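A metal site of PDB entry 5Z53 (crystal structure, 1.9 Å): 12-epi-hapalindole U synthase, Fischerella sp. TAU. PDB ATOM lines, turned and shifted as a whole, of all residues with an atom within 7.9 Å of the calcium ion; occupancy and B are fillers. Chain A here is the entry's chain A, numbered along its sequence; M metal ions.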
ATOM      1  N   ASN A  35     -24.072  32.612  15.458  1.00  0.00           N
ATOM      2  CA  ASN A  35     -23.541  31.824  14.385  1.00  0.00           C
ATOM      3  C   ASN A  35     -24.708  31.166  13.624  1.00  0.00           C
ATOM      4  O   ASN A  35     -24.656  29.961  13.306  1.00  0.00           O
ATOM      5  CB  ASN A  35     -22.549  30.780  14.878  1.00  0.00           C
ATOM      6  CG  ASN A  35     -21.585  30.301  13.810  1.00  0.00           C
ATOM      7  OD1 ASN A  35     -21.441  30.910  12.744  1.00  0.00           O
ATOM      8  ND2 ASN A  35     -20.921  29.196  14.080  1.00  0.00           N
ATOM      9  N   ALA A  36     -25.724  31.981  13.322  1.00  0.00           N
ATOM     10  CA  ALA A  36     -27.007  31.522  12.843  1.00  0.00           C
ATOM     11  C   ALA A  36     -26.913  30.943  11.441  1.00  0.00           C
ATOM     12  O   ALA A  36     -27.731  30.118  11.069  1.00  0.00           O
ATOM     13  CB  ALA A  36     -28.022  32.638  12.942  1.00  0.00           C
ATOM     14  N   GLY A  37     -25.897  31.345  10.659  1.00  0.00           N
ATOM     15  CA  GLY A  37     -25.662  30.794   9.313  1.00  0.00           C
ATOM     16  C   GLY A  37     -24.363  30.007   9.198  1.00  0.00           C
ATOM     17  O   GLY A  37     -23.832  29.802   8.122  1.00  0.00           O
ATOM     18  N   PHE A  38     -23.819  29.566  10.345  1.00  0.00           N
ATOM     19  CA  PHE A  38     -22.641  28.734  10.411  1.00  0.00           C
ATOM     20  C   PHE A  38     -21.434  29.320   9.674  1.00  0.00           C
ATOM     21  O   PHE A  38     -20.609  28.587   9.167  1.00  0.00           O
ATOM     22  CB  PHE A  38     -22.959  27.324   9.893  1.00  0.00           C
ATOM     23  CG  PHE A  38     -24.049  26.641  10.695  1.00  0.00           C
ATOM     24  CD1 PHE A  38     -23.747  26.010  11.888  1.00  0.00           C
ATOM     25  CD2 PHE A  38     -25.347  26.552  10.203  1.00  0.00           C
ATOM     26  CE1 PHE A  38     -24.743  25.362  12.606  1.00  0.00           C
ATOM     27  CE2 PHE A  38     -26.351  25.972  10.947  1.00  0.00           C
ATOM     28  CZ  PHE A  38     -26.036  25.345  12.143  1.00  0.00           C
ATOM     29  N   GLU A  39     -21.321  30.660   9.663  1.00  0.00           N
ATOM     30  CA  GLU A  39     -20.262  31.302   8.912  1.00  0.00           C
ATOM     31  C   GLU A  39     -18.941  31.277   9.700  1.00  0.00           C
ATOM     32  O   GLU A  39     -17.881  31.423   9.097  1.00  0.00           O
ATOM     33  CB  GLU A  39     -20.667  32.726   8.521  1.00  0.00           C
ATOM     34  CG  GLU A  39     -21.805  32.753   7.511  1.00  0.00           C
ATOM     35  CD  GLU A  39     -21.515  32.042   6.194  1.00  0.00           C
ATOM     36  OE1 GLU A  39     -20.471  32.348   5.553  1.00  0.00           O
ATOM     37  OE2 GLU A  39     -22.246  31.095   5.854  1.00  0.00           O
ATOM     38  N   ASP A  40     -18.966  30.972  11.003  1.00  0.00           N
ATOM     39  CA  ASP A  40     -17.748  30.669  11.763  1.00  0.00           C
ATOM     40  C   ASP A  40     -17.680  29.140  11.933  1.00  0.00           C
ATOM     41  O   ASP A  40     -18.661  28.545  12.399  1.00  0.00           O
ATOM     42  CB  ASP A  40     -17.733  31.384  13.120  1.00  0.00           C
ATOM     43  CG  ASP A  40     -17.161  32.803  13.080  1.00  0.00           C
ATOM     44  OD1 ASP A  40     -16.699  33.202  12.008  1.00  0.00           O
ATOM     45  OD2 ASP A  40     -17.114  33.492  14.132  1.00  0.00           O
ATOM     46  N   GLY A  80     -19.379  23.366   6.552  1.00  0.00           N
ATOM     47  CA  GLY A  80     -18.854  22.967   5.270  1.00  0.00           C
ATOM     48  C   GLY A  80     -19.075  24.102   4.278  1.00  0.00           C
ATOM     49  O   GLY A  80     -20.107  24.761   4.410  1.00  0.00           O
ATOM     50  N   ALA A  93     -24.542  27.729  -0.924  1.00  0.00           N
ATOM     51  CA  ALA A  93     -25.124  27.810   0.409  1.00  0.00           C
ATOM     52  C   ALA A  93     -26.304  28.769   0.300  1.00  0.00           C
ATOM     53  O   ALA A  93     -26.195  29.807  -0.356  1.00  0.00           O
ATOM     54  CB  ALA A  93     -24.132  28.350   1.417  1.00  0.00           C
ATOM     55  N   PRO A  94     -27.419  28.480   1.001  1.00  0.00           N
ATOM     56  CA  PRO A  94     -28.532  29.427   1.109  1.00  0.00           C
ATOM     57  C   PRO A  94     -28.089  30.798   1.605  1.00  0.00           C
ATOM     58  O   PRO A  94     -28.665  31.793   1.205  1.00  0.00           O
ATOM     59  CB  PRO A  94     -29.501  28.749   2.091  1.00  0.00           C
ATOM     60  CG  PRO A  94     -29.229  27.299   1.839  1.00  0.00           C
ATOM     61  CD  PRO A  94     -27.746  27.175   1.592  1.00  0.00           C
ATOM     62  N   GLU A  95     -27.041  30.848   2.439  1.00  0.00           N
ATOM     63  CA  GLU A  95     -26.608  32.092   3.052  1.00  0.00           C
ATOM     64  C   GLU A  95     -25.093  32.047   3.207  1.00  0.00           C
ATOM     65  O   GLU A  95     -24.527  31.091   3.719  1.00  0.00           O
ATOM     66  CB  GLU A  95     -27.347  32.324   4.384  1.00  0.00           C
ATOM     67  CG  GLU A  95     -26.845  33.552   5.168  1.00  0.00           C
ATOM     68  CD  GLU A  95     -25.592  33.409   6.037  1.00  0.00           C
ATOM     69  OE1 GLU A  95     -24.987  34.468   6.415  1.00  0.00           O
ATOM     70  OE2 GLU A  95     -25.184  32.261   6.375  1.00  0.00           O
ATOM     71  N   GLY A  96     -24.419  33.103   2.752  1.00  0.00           N
ATOM     72  CA  GLY A  96     -22.956  33.225   2.884  1.00  0.00           C
ATOM     73  C   GLY A  96     -22.223  32.058   2.220  1.00  0.00           C
ATOM     74  O   GLY A  96     -22.645  31.569   1.173  1.00  0.00           O
ATOM     75  N   ARG A  97     -21.170  31.564   2.894  1.00  0.00           N
ATOM     76  CA  ARG A  97     -20.255  30.561   2.370  1.00  0.00           C
ATOM     77  C   ARG A  97     -20.576  29.153   2.842  1.00  0.00           C
ATOM     78  O   ARG A  97     -20.553  28.180   2.048  1.00  0.00           O
ATOM     79  CB  ARG A  97     -18.826  30.881   2.794  1.00  0.00           C
ATOM     80  CG  ARG A  97     -18.223  32.125   2.155  1.00  0.00           C
ATOM     81  CD  ARG A  97     -16.932  32.427   2.890  1.00  0.00           C
ATOM     82  NE  ARG A  97     -15.846  31.538   2.503  1.00  0.00           N
ATOM     83  CZ  ARG A  97     -15.056  31.688   1.415  1.00  0.00           C
ATOM     84  NH1 ARG A  97     -15.200  32.695   0.566  1.00  0.00           N
ATOM     85  NH2 ARG A  97     -14.014  30.881   1.277  1.00  0.00           N
ATOM     86  N   ASN A  98     -21.070  29.066   4.075  1.00  0.00           N
ATOM     87  CA  ASN A  98     -21.058  27.801   4.793  1.00  0.00           C
ATOM     88  C   ASN A  98     -22.464  27.324   5.109  1.00  0.00           C
ATOM     89  O   ASN A  98     -23.389  28.135   5.313  1.00  0.00           O
ATOM     90  CB  ASN A  98     -20.380  27.976   6.159  1.00  0.00           C
ATOM     91  CG  ASN A  98     -18.882  28.200   6.086  1.00  0.00           C
ATOM     92  OD1 ASN A  98     -18.253  27.965   5.046  1.00  0.00           O
ATOM     93  ND2 ASN A  98     -18.305  28.594   7.206  1.00  0.00           N
ATOM     94  N   ILE A  99     -22.522  25.996   5.350  1.00  0.00           N
ATOM     95  CA  ILE A  99     -23.614  25.347   5.999  1.00  0.00           C
ATOM     96  C   ILE A  99     -23.111  24.649   7.284  1.00  0.00           C
ATOM     97  O   ILE A  99     -21.904  24.514   7.513  1.00  0.00           O
ATOM     98  CB  ILE A  99     -24.284  24.401   4.990  1.00  0.00           C
ATOM     99  CG1 ILE A  99     -23.388  23.291   4.420  1.00  0.00           C
ATOM    100  CG2 ILE A  99     -24.791  25.260   3.824  1.00  0.00           C
ATOM    101  CD1 ILE A  99     -23.008  22.160   5.368  1.00  0.00           C
ATOM    102  N   GLY A 100     -24.057  24.186   8.105  1.00  0.00           N
ATOM    103  CA  GLY A 100     -23.749  23.246   9.231  1.00  0.00           C
ATOM    104  C   GLY A 100     -24.257  21.873   8.847  1.00  0.00           C
ATOM    105  O   GLY A 100     -25.409  21.723   8.393  1.00  0.00           O
ATOM    106  N   PHE A 215     -27.766  22.147   7.176  1.00  0.00           N
ATOM    107  CA  PHE A 215     -28.673  23.171   7.605  1.00  0.00           C
ATOM    108  C   PHE A 215     -28.036  24.545   7.375  1.00  0.00           C
ATOM    109  O   PHE A 215     -26.829  24.654   7.377  1.00  0.00           O
ATOM    110  CB  PHE A 215     -28.926  23.043   9.090  1.00  0.00           C
ATOM    111  CG  PHE A 215     -29.703  21.822   9.487  1.00  0.00           C
ATOM    112  CD1 PHE A 215     -31.070  21.800   9.377  1.00  0.00           C
ATOM    113  CD2 PHE A 215     -29.057  20.724  10.026  1.00  0.00           C
ATOM    114  CE1 PHE A 215     -31.802  20.679   9.779  1.00  0.00           C
ATOM    115  CE2 PHE A 215     -29.775  19.592  10.414  1.00  0.00           C
ATOM    116  CZ  PHE A 215     -31.153  19.594  10.317  1.00  0.00           C
ATOM    117  N   ASP A 216     -28.837  25.585   7.154  1.00  0.00           N
ATOM    118  CA  ASP A 216     -28.294  26.943   6.972  1.00  0.00           C
ATOM    119  C   ASP A 216     -29.373  28.001   7.212  1.00  0.00           C
ATOM    120  O   ASP A 216     -30.542  27.699   7.239  1.00  0.00           O
ATOM    121  CB  ASP A 216     -27.672  27.140   5.594  1.00  0.00           C
ATOM    122  CG  ASP A 216     -26.717  28.329   5.528  1.00  0.00           C
ATOM    123  OD1 ASP A 216     -26.324  28.847   6.595  1.00  0.00           O
ATOM    124  OD2 ASP A 216     -26.297  28.681   4.405  1.00  0.00           O
ATOM    125  N   ASN A 217     -28.909  29.213   7.544  1.00  0.00           N
ATOM    126  CA  ASN A 217     -29.720  30.387   7.574  1.00  0.00           C
ATOM    127  C   ASN A 217     -30.860  30.247   8.586  1.00  0.00           C
ATOM    128  O   ASN A 217     -32.025  30.381   8.247  1.00  0.00           O
ATOM    129  CB  ASN A 217     -30.207  30.736   6.163  1.00  0.00           C
ATOM    130  CG  ASN A 217     -30.727  32.153   6.104  1.00  0.00           C
ATOM    131  OD1 ASN A 217     -30.351  32.996   6.914  1.00  0.00           O
ATOM    132  ND2 ASN A 217     -31.620  32.398   5.147  1.00  0.00           N
ATOM    133  N   VAL A 218     -30.490  30.047   9.855  1.00  0.00           N
ATOM    134  CA  VAL A 218     -31.447  29.875  10.898  1.00  0.00           C
ATOM    135  C   VAL A 218     -31.978  31.238  11.288  1.00  0.00           C
ATOM    136  O   VAL A 218     -31.194  32.153  11.613  1.00  0.00           O
ATOM    137  CB  VAL A 218     -30.859  29.194  12.140  1.00  0.00           C
ATOM    138  CG1 VAL A 218     -31.908  28.938  13.190  1.00  0.00           C
ATOM    139  CG2 VAL A 218     -30.118  27.931  11.778  1.00  0.00           C
HETATM  140 CA    CA M   1     -24.418  30.103   5.841  1.00  0.00          CA
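The backbone NH of Glu 39 sits at hydrogen-bond distance from the side-chain amide oxygen of Asn 35 (3.1 Å).
ND2 of Asn 98 lies within hydrogen-bond range of O of Phe 38.
N of Arg 97 lies within hydrogen-bond range of OE1 of Glu 39, 2.9 Å away.
Of the 19 residues printed, 5 come within 4 Å of the calcium ion.
The calcium ion is bound by the backbone carbonyl oxygen (O) of Asn 98 (2.3 Å), the backbone carbonyl oxygen (O) of Glu 95 (2.3 Å), the side-chain carboxylate (OE2) of Glu 95 (2.4 Å), the backbone carbonyl oxygen (O) of Gly 37 (2.4 Å), the side-chain carboxylate (OE2) of Glu 39 (2.4 Å), the side-chain carboxylate (OD1) of Asp 216 (2.4 Å) and the side-chain carboxylate (OD2) of Asp 216 (2.8 Å).
The calcium ion has seven donor atoms within binding distance.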
